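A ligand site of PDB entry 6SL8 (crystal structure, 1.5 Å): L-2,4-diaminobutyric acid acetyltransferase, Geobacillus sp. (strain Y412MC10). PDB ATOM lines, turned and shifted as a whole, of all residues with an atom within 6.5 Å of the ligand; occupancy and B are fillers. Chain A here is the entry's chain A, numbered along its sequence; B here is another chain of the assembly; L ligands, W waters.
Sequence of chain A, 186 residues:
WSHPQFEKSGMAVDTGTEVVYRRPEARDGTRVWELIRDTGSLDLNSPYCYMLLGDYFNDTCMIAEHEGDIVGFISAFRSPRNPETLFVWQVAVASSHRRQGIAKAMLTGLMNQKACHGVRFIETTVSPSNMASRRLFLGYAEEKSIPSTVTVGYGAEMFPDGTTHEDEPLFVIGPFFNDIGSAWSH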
ATOM      1  N   ILE A  36       7.040   5.427  -9.866  1.00  0.00           N
ATOM      2  CA  ILE A  36       7.862   4.558  -9.059  1.00  0.00           C
ATOM      3  C   ILE A  36       8.082   5.219  -7.694  1.00  0.00           C
ATOM      4  O   ILE A  36       8.107   4.540  -6.663  1.00  0.00           O
ATOM      5  CB  ILE A  36       9.241   4.222  -9.714  1.00  0.00           C
ATOM      6  CG1 ILE A  36       9.017   3.690 -11.152  1.00  0.00           C
ATOM      7  CG2 ILE A  36      10.024   3.239  -8.893  1.00  0.00           C
ATOM      8  CD1 ILE A  36       8.131   2.465 -11.235  1.00  0.00           C
ATOM      9  N   SER A  41       7.026   0.313  -2.196  1.00  0.00           N
ATOM     10  CA  SER A  41       7.529  -1.068  -2.248  1.00  0.00           C
ATOM     11  C   SER A  41       8.721  -1.240  -3.205  1.00  0.00           C
ATOM     12  O   SER A  41       9.439  -2.203  -3.093  1.00  0.00           O
ATOM     13  CB  SER A  41       6.438  -2.053  -2.664  1.00  0.00           C
ATOM     14  OG  SER A  41       5.864  -1.759  -3.941  1.00  0.00           O
ATOM     15  N   LEU A  42       8.868  -0.321  -4.132  1.00  0.00           N
ATOM     16  CA  LEU A  42       9.897  -0.448  -5.134  1.00  0.00           C
ATOM     17  C   LEU A  42      11.135   0.416  -4.767  1.00  0.00           C
ATOM     18  O   LEU A  42      11.027   1.451  -4.098  1.00  0.00           O
ATOM     19  CB  LEU A  42       9.371  -0.019  -6.530  1.00  0.00           C
ATOM     20  CG  LEU A  42       8.276  -0.897  -7.146  1.00  0.00           C
ATOM     21  CD1 LEU A  42       7.776  -0.225  -8.398  1.00  0.00           C
ATOM     22  CD2 LEU A  42       8.815  -2.283  -7.417  1.00  0.00           C
ATOM     23  N   ASP A  43      12.297   0.011  -5.294  1.00  0.00           N
ATOM     24  CA  ASP A  43      13.534   0.782  -5.213  1.00  0.00           C
ATOM     25  C   ASP A  43      13.660   1.800  -6.327  1.00  0.00           C
ATOM     26  O   ASP A  43      13.542   1.460  -7.522  1.00  0.00           O
ATOM     27  CB  ASP A  43      14.721  -0.138  -5.239  1.00  0.00           C
ATOM     28  CG  ASP A  43      14.732  -1.104  -4.068  1.00  0.00           C
ATOM     29  OD1 ASP A  43      14.261  -0.728  -2.955  1.00  0.00           O
ATOM     30  OD2 ASP A  43      15.107  -2.245  -4.287  1.00  0.00           O
ATOM     31  N   LEU A  44      13.733   3.090  -6.024  1.00  0.00           N
ATOM     32  CA  LEU A  44      13.661   4.084  -7.042  1.00  0.00           C
ATOM     33  C   LEU A  44      15.034   4.209  -7.769  1.00  0.00           C
ATOM     34  O   LEU A  44      16.070   4.424  -7.181  1.00  0.00           O
ATOM     35  CB  LEU A  44      13.281   5.430  -6.381  1.00  0.00           C
ATOM     36  CG  LEU A  44      13.096   6.602  -7.293  1.00  0.00           C
ATOM     37  CD1 LEU A  44      11.992   6.417  -8.277  1.00  0.00           C
ATOM     38  CD2 LEU A  44      12.859   7.881  -6.437  1.00  0.00           C
ATOM     39  N   ASN A  45      14.980   4.088  -9.104  1.00  0.00           N
ATOM     40  CA  ASN A  45      16.148   4.382  -9.930  1.00  0.00           C
ATOM     41  C   ASN A  45      16.115   5.846 -10.387  1.00  0.00           C
ATOM     42  O   ASN A  45      15.195   6.595 -10.104  1.00  0.00           O
ATOM     43  CB  ASN A  45      16.228   3.386 -11.088  1.00  0.00           C
ATOM     44  CG  ASN A  45      16.323   1.976 -10.561  1.00  0.00           C
ATOM     45  OD1 ASN A  45      15.312   1.169 -10.644  1.00  0.00           O
ATOM     46  ND2 ASN A  45      17.366   1.669  -9.997  1.00  0.00           N
ATOM     47  N   TYR A  50      14.718   5.398 -16.392  1.00  0.00           N
ATOM     48  CA  TYR A  50      13.420   5.202 -17.022  1.00  0.00           C
ATOM     49  C   TYR A  50      13.301   5.760 -18.440  1.00  0.00           C
ATOM     50  O   TYR A  50      12.521   5.182 -19.258  1.00  0.00           O
ATOM     51  CB  TYR A  50      12.238   5.715 -16.088  1.00  0.00           C
ATOM     52  CG  TYR A  50      12.270   5.005 -14.728  1.00  0.00           C
ATOM     53  CD1 TYR A  50      11.897   3.668 -14.628  1.00  0.00           C
ATOM     54  CD2 TYR A  50      12.853   5.585 -13.636  1.00  0.00           C
ATOM     55  CE1 TYR A  50      12.041   2.976 -13.454  1.00  0.00           C
ATOM     56  CE2 TYR A  50      12.984   4.894 -12.427  1.00  0.00           C
ATOM     57  CZ  TYR A  50      12.581   3.574 -12.370  1.00  0.00           C
ATOM     58  OH  TYR A  50      12.739   2.845 -11.203  1.00  0.00           O
ATOM     59  N   PHE A  87      13.056 -11.261 -17.988  1.00  0.00           N
ATOM     60  CA  PHE A  87      13.241 -10.792 -16.584  1.00  0.00           C
ATOM     61  C   PHE A  87      12.343  -9.638 -16.353  1.00  0.00           C
ATOM     62  O   PHE A  87      12.489  -8.598 -17.044  1.00  0.00           O
ATOM     63  CB  PHE A  87      14.693 -10.459 -16.311  1.00  0.00           C
ATOM     64  CG  PHE A  87      14.897 -10.102 -14.837  1.00  0.00           C
ATOM     65  CD1 PHE A  87      15.127 -11.110 -13.968  1.00  0.00           C
ATOM     66  CD2 PHE A  87      14.716  -8.814 -14.360  1.00  0.00           C
ATOM     67  CE1 PHE A  87      15.242 -10.867 -12.590  1.00  0.00           C
ATOM     68  CE2 PHE A  87      14.854  -8.564 -12.968  1.00  0.00           C
ATOM     69  CZ  PHE A  87      15.096  -9.604 -12.146  1.00  0.00           C
ATOM     70  N   VAL A  88      11.440  -9.730 -15.380  1.00  0.00           N
ATOM     71  CA  VAL A  88      10.542  -8.691 -14.979  1.00  0.00           C
ATOM     72  C   VAL A  88      11.172  -7.951 -13.838  1.00  0.00           C
ATOM     73  O   VAL A  88      11.412  -8.519 -12.746  1.00  0.00           O
ATOM     74  CB  VAL A  88       9.088  -9.124 -14.717  1.00  0.00           C
ATOM     75  CG1 VAL A  88       8.279  -7.965 -14.261  1.00  0.00           C
ATOM     76  CG2 VAL A  88       8.518  -9.803 -15.965  1.00  0.00           C
ATOM     77  N   TRP A  89      11.435  -6.640 -14.024  1.00  0.00           N
ATOM     78  CA  TRP A  89      12.211  -5.852 -13.107  1.00  0.00           C
ATOM     79  C   TRP A  89      11.284  -5.138 -12.116  1.00  0.00           C
ATOM     80  O   TRP A  89      11.392  -5.418 -10.906  1.00  0.00           O
ATOM     81  CB  TRP A  89      13.102  -4.885 -13.864  1.00  0.00           C
ATOM     82  CG  TRP A  89      14.033  -4.036 -13.111  1.00  0.00           C
ATOM     83  CD1 TRP A  89      14.141  -3.967 -11.733  1.00  0.00           C
ATOM     84  CD2 TRP A  89      14.961  -3.103 -13.642  1.00  0.00           C
ATOM     85  NE1 TRP A  89      15.073  -3.011 -11.421  1.00  0.00           N
ATOM     86  CE2 TRP A  89      15.635  -2.495 -12.583  1.00  0.00           C
ATOM     87  CE3 TRP A  89      15.289  -2.742 -14.968  1.00  0.00           C
ATOM     88  CZ2 TRP A  89      16.609  -1.480 -12.799  1.00  0.00           C
ATOM     89  CZ3 TRP A  89      16.267  -1.744 -15.196  1.00  0.00           C
ATOM     90  CH2 TRP A  89      16.930  -1.176 -14.116  1.00  0.00           C
ATOM     91  N   GLN A  90      10.469  -4.212 -12.537  1.00  0.00           N
ATOM     92  CA  GLN A  90       9.602  -3.473 -11.623  1.00  0.00           C
ATOM     93  C   GLN A  90       8.165  -3.556 -12.134  1.00  0.00           C
ATOM     94  O   GLN A  90       7.930  -3.295 -13.310  1.00  0.00           O
ATOM     95  CB  GLN A  90      10.004  -2.020 -11.381  1.00  0.00           C
ATOM     96  CG  GLN A  90      11.393  -1.930 -10.826  1.00  0.00           C
ATOM     97  CD  GLN A  90      11.788  -0.499 -10.468  1.00  0.00           C
ATOM     98  OE1 GLN A  90      11.883   0.369 -11.333  1.00  0.00           O
ATOM     99  NE2 GLN A  90      12.105  -0.289  -9.222  1.00  0.00           N
ATOM    100  N   VAL A  91       7.209  -3.784 -11.238  1.00  0.00           N
ATOM    101  CA  VAL A  91       5.754  -3.704 -11.473  1.00  0.00           C
ATOM    102  C   VAL A  91       5.179  -2.650 -10.516  1.00  0.00           C
ATOM    103  O   VAL A  91       5.322  -2.790  -9.296  1.00  0.00           O
ATOM    104  CB  VAL A  91       5.091  -5.102 -11.254  1.00  0.00           C
ATOM    105  CG1 VAL A  91       3.601  -4.997 -11.457  1.00  0.00           C
ATOM    106  CG2 VAL A  91       5.785  -6.219 -12.019  1.00  0.00           C
ATOM    107  N   THR A 124      11.897 -13.167 -11.975  1.00  0.00           N
ATOM    108  CA  THR A 124      11.615 -11.934 -11.328  1.00  0.00           C
ATOM    109  C   THR A 124      11.991 -12.101  -9.884  1.00  0.00           C
ATOM    110  O   THR A 124      12.068 -13.262  -9.471  1.00  0.00           O
ATOM    111  CB  THR A 124      10.172 -11.461 -11.499  1.00  0.00           C
ATOM    112  OG1 THR A 124       9.956 -10.095 -11.122  1.00  0.00           O
ATOM    113  CG2 THR A 124       9.162 -12.396 -10.811  1.00  0.00           C
ATOM    114  N   THR A 125      12.152 -11.033  -9.152  1.00  0.00           N
ATOM    115  CA  THR A 125      12.333 -11.231  -7.697  1.00  0.00           C
ATOM    116  C   THR A 125      11.179 -10.527  -7.008  1.00  0.00           C
ATOM    117  O   THR A 125      10.670  -9.439  -7.409  1.00  0.00           O
ATOM    118  CB  THR A 125      13.727 -10.764  -7.129  1.00  0.00           C
ATOM    119  OG1 THR A 125      13.815  -9.345  -7.176  1.00  0.00           O
ATOM    120  CG2 THR A 125      14.872 -11.352  -7.756  1.00  0.00           C
ATOM    121  N   VAL A 126      10.695 -11.149  -5.884  1.00  0.00           N
ATOM    122  CA  VAL A 126       9.532 -10.642  -5.194  1.00  0.00           C
ATOM    123  C   VAL A 126       9.812 -10.708  -3.665  1.00  0.00           C
ATOM    124  O   VAL A 126       9.761 -11.815  -3.140  1.00  0.00           O
ATOM    125  CB  VAL A 126       8.214 -11.428  -5.492  1.00  0.00           C
ATOM    126  CG1 VAL A 126       7.028 -10.762  -4.901  1.00  0.00           C
ATOM    127  CG2 VAL A 126       8.046 -11.512  -7.042  1.00  0.00           C
ATOM    128  N   SER A 127       9.953  -9.562  -3.058  1.00  0.00           N
ATOM    129  CA  SER A 127      10.293  -9.579  -1.562  1.00  0.00           C
ATOM    130  C   SER A 127       9.033 -10.079  -0.859  1.00  0.00           C
ATOM    131  O   SER A 127       7.834  -9.937  -1.296  1.00  0.00           O
ATOM    132  CB  SER A 127      10.652  -8.165  -1.113  1.00  0.00           C
ATOM    133  OG  SER A 127      11.926  -7.782  -1.598  1.00  0.00           O
ATOM    134  N   ASN A 130       5.767  -8.115  -0.582  1.00  0.00           N
ATOM    135  CA  ASN A 130       5.139  -7.767  -1.852  1.00  0.00           C
ATOM    136  C   ASN A 130       4.043  -8.770  -2.235  1.00  0.00           C
ATOM    137  O   ASN A 130       4.177  -9.517  -3.216  1.00  0.00           O
ATOM    138  CB  ASN A 130       6.164  -7.628  -2.970  1.00  0.00           C
ATOM    139  CG  ASN A 130       7.110  -6.396  -2.862  1.00  0.00           C
ATOM    140  OD1 ASN A 130       7.487  -5.889  -1.780  1.00  0.00           O
ATOM    141  ND2 ASN A 130       7.571  -5.965  -3.992  1.00  0.00           N
ATOM    142  N   HIS A 165      16.978  -3.452   3.704  1.00  0.00           N
ATOM    143  CA  HIS A 165      16.340  -4.082   2.530  1.00  0.00           C
ATOM    144  C   HIS A 165      15.915  -5.522   2.878  1.00  0.00           C
ATOM    145  O   HIS A 165      16.654  -6.256   3.529  1.00  0.00           O
ATOM    146  CB  HIS A 165      17.331  -4.103   1.328  1.00  0.00           C
ATOM    147  CG  HIS A 165      16.643  -4.096  -0.030  1.00  0.00           C
ATOM    148  ND1 HIS A 165      16.044  -5.202  -0.580  1.00  0.00           N
ATOM    149  CD2 HIS A 165      16.431  -3.080  -0.904  1.00  0.00           C
ATOM    150  CE1 HIS A 165      15.520  -4.863  -1.764  1.00  0.00           C
ATOM    151  NE2 HIS A 165      15.745  -3.583  -1.973  1.00  0.00           N
ATOM    152  N   GLU A 168      15.270 -10.589  -1.691  1.00  0.00           N
ATOM    153  CA  GLU A 168      14.632 -10.573  -3.052  1.00  0.00           C
ATOM    154  C   GLU A 168      14.733 -11.984  -3.608  1.00  0.00           C
ATOM    155  O   GLU A 168      15.610 -12.319  -4.405  1.00  0.00           O
ATOM    156  CB  GLU A 168      15.460  -9.600  -3.916  1.00  0.00           C
ATOM    157  CG  GLU A 168      15.274  -8.135  -3.613  1.00  0.00           C
ATOM    158  CD  GLU A 168      14.005  -7.547  -4.096  1.00  0.00           C
ATOM    159  OE1 GLU A 168      13.172  -8.231  -4.855  1.00  0.00           O
ATOM    160  OE2 GLU A 168      13.761  -6.350  -3.794  1.00  0.00           O
ATOM    161  N   SER B  46      19.450   2.487  -8.018  1.00  0.00           N
ATOM    162  CA  SER B  46      19.352   1.608  -6.831  1.00  0.00           C
ATOM    163  C   SER B  46      20.452   0.627  -6.816  1.00  0.00           C
ATOM    164  O   SER B  46      20.962   0.163  -7.830  1.00  0.00           O
ATOM    165  CB  SER B  46      17.971   0.884  -6.795  1.00  0.00           C
ATOM    166  OG  SER B  46      17.883  -0.041  -7.839  1.00  0.00           O
ATOM    167  N   TYR B  48      19.971  -2.484  -6.259  1.00  0.00           N
ATOM    168  CA  TYR B  48      19.391  -3.588  -7.043  1.00  0.00           C
ATOM    169  C   TYR B  48      19.711  -3.503  -8.541  1.00  0.00           C
ATOM    170  O   TYR B  48      20.037  -4.516  -9.186  1.00  0.00           O
ATOM    171  CB  TYR B  48      17.894  -3.639  -6.776  1.00  0.00           C
ATOM    172  CG  TYR B  48      17.189  -4.804  -7.404  1.00  0.00           C
ATOM    173  CD1 TYR B  48      16.803  -4.833  -8.723  1.00  0.00           C
ATOM    174  CD2 TYR B  48      16.883  -5.925  -6.643  1.00  0.00           C
ATOM    175  CE1 TYR B  48      16.096  -5.890  -9.229  1.00  0.00           C
ATOM    176  CE2 TYR B  48      16.165  -6.985  -7.156  1.00  0.00           C
ATOM    177  CZ  TYR B  48      15.786  -6.942  -8.504  1.00  0.00           C
ATOM    178  OH  TYR B  48      15.087  -7.997  -9.064  1.00  0.00           O
ATOM    179  N   CYS B  49      19.635  -2.296  -9.097  1.00  0.00           N
ATOM    180  CA  CYS B  49      20.025  -2.045 -10.531  1.00  0.00           C
ATOM    181  C   CYS B  49      21.406  -2.585 -10.804  1.00  0.00           C
ATOM    182  O   CYS B  49      21.647  -3.316 -11.772  1.00  0.00           O
ATOM    183  CB  CYS B  49      19.960  -0.546 -10.748  1.00  0.00           C
ATOM    184  SG  CYS B  49      20.371  -0.106 -12.498  1.00  0.00           S
ATOM    185  N   LEU B  52      21.514  -6.356 -10.819  1.00  0.00           N
ATOM    186  CA  LEU B  52      21.001  -6.815 -12.100  1.00  0.00           C
ATOM    187  C   LEU B  52      21.993  -6.739 -13.234  1.00  0.00           C
ATOM    188  O   LEU B  52      22.101  -7.631 -14.112  1.00  0.00           O
ATOM    189  CB  LEU B  52      19.731  -6.054 -12.529  1.00  0.00           C
ATOM    190  CG  LEU B  52      18.442  -6.277 -11.935  1.00  0.00           C
ATOM    191  CD1 LEU B  52      17.428  -5.515 -12.841  1.00  0.00           C
ATOM    192  CD2 LEU B  52      18.055  -7.757 -11.851  1.00  0.00           C
HETATM  193  N1  LIG L   1      12.841  -4.321  -5.320  1.00  0.00           N
HETATM  194  C1  LIG L   1      13.333  -4.399  -6.752  1.00  0.00           C
HETATM  195  C2  LIG L   1      13.099  -3.100  -7.435  1.00  0.00           C
HETATM  196  O1  LIG L   1      12.311  -2.316  -7.009  1.00  0.00           O
HETATM  197  C3  LIG L   1      12.834  -5.644  -7.484  1.00  0.00           C
HETATM  198  C4  LIG L   1      11.398  -5.489  -7.740  1.00  0.00           C
HETATM  199  N2  LIG L   1      10.873  -6.731  -8.351  1.00  0.00           N
HETATM  200  O2  LIG L   1      13.788  -2.934  -8.479  1.00  0.00           O
HETATM  201  O   HOH W   1      12.479  -8.262 -10.207  1.00  0.00           O
HETATM  202  O   HOH W   2      10.002  -4.538  -4.534  1.00  0.00           O
HETATM  203  O   HOH W   3       8.162  -5.705  -9.059  1.00  0.00           O
HETATM  204  O   HOH W   4       8.303  -7.665  -6.552  1.00  0.00           O
HETATM  205  O   HOH W   5      12.329  -2.833  -2.887  1.00  0.00           O
HETATM  206  O   HOH W   6      10.604  -7.321  -4.872  1.00  0.00           O
HETATM  207  O   HOH W   7       8.456  -8.557  -9.274  1.00  0.00           O
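Water W1 lies within hydrogen-bond range of the backbone carbonyl oxygen (O) of Val 88, the side-chain hydroxyl (OH) of Tyr 48 of chain B, a nitrogen (N2) of the ligand, the backbone NH (N) of Thr 125, the backbone carbonyl oxygen (O) of Trp 89 and the side-chain hydroxyl (OG1) of Thr 124.
Water W5 lies within hydrogen-bond range of OD1 of Asp 43 (2.9 Å), N1 of the ligand (2.9 Å) and O of Ser 41 (3.0 Å).
Water W2 lies within hydrogen-bond range of the backbone carbonyl oxygen of Ser 41 (2.8 Å), the side-chain amide nitrogen of Asn 130 (2.9 Å) and a nitrogen (N1) of the ligand (3.0 Å).
Water W3 bridges N2 of the ligand and N of Val 91.
Water W7 lies within hydrogen-bond range of the side-chain hydroxyl (OG1) of Thr 124, the backbone carbonyl oxygen (O) of Thr 125 and a nitrogen (N2) of the ligand.
Water W4 lies within hydrogen-bond range of the backbone carbonyl oxygen (O) of Thr 125 (3.1 Å), the side-chain amide nitrogen (ND2) of Asn 130 (3.2 Å) and a nitrogen (N2) of the ligand (3.3 Å).
The side-chain amide oxygen (OE1) of Gln 90 sits at hydrogen-bond distance from the side-chain hydroxyl (OH) of Tyr 50 (2.6 Å).
OG1 of Thr 125 sits at hydrogen-bond distance from OE1 of Glu 168, at 2.7 Å.
The side-chain carboxylate of Asp 43 lies within hydrogen-bond range of a ring nitrogen (NE2) of His 165.
The side-chain hydroxyl (OG) of Ser 127 lies within hydrogen-bond range of the side-chain carboxylate (OE2) of Glu 168 (3.2 Å).
The side-chain amide nitrogen (NE2) of Gln 90 is in hydrogen-bond range of the backbone carbonyl oxygen (O) of Asp 43 (2.8 Å).
The side-chain hydroxyl of Thr 125 lies within hydrogen-bond range of the side-chain hydroxyl of Tyr 48 of chain B.
The backbone carbonyl oxygen of Thr 125 lies within hydrogen-bond range of a nitrogen (N2) of the ligand, at 2.9 Å.
The side-chain carboxylate (OD2) of Asp 43 is in salt-bridge range of a nitrogen (N1) of the ligand (3.2 Å).
The side-chain carboxylate (OE2) of Glu 168 is in salt-bridge range of a nitrogen (N1) of the ligand (2.7 Å).
An oxygen (O1) of the ligand sits at hydrogen-bond distance from the backbone NH (N) of Asp 43 (2.9 Å).
An oxygen (O1) of the ligand is in hydrogen-bond range of the side-chain amide nitrogen (NE2) of Gln 90, at 3.0 Å.
The indole nitrogen of Trp 89 sits at hydrogen-bond distance from an oxygen (O2) of the ligand (3.2 Å).
The backbone carbonyl oxygen of Trp 89 is in hydrogen-bond range of a nitrogen (N2) of the ligand (2.9 Å).
Leu 42 touches the ligand (CD2 to O1, 3.5 Å).
Tyr 48 of chain B touches the ligand.
Hydrophobic or aromatic side chains within 4 Å of the ligand: Leu 42, Trp 89 and Tyr 48 of chain B.
Of the 23 residues printed, 7 come within 4 Å of the ligand.
The nearest printed residue that does not touch the ligand is Thr 124 (4.5 Å).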
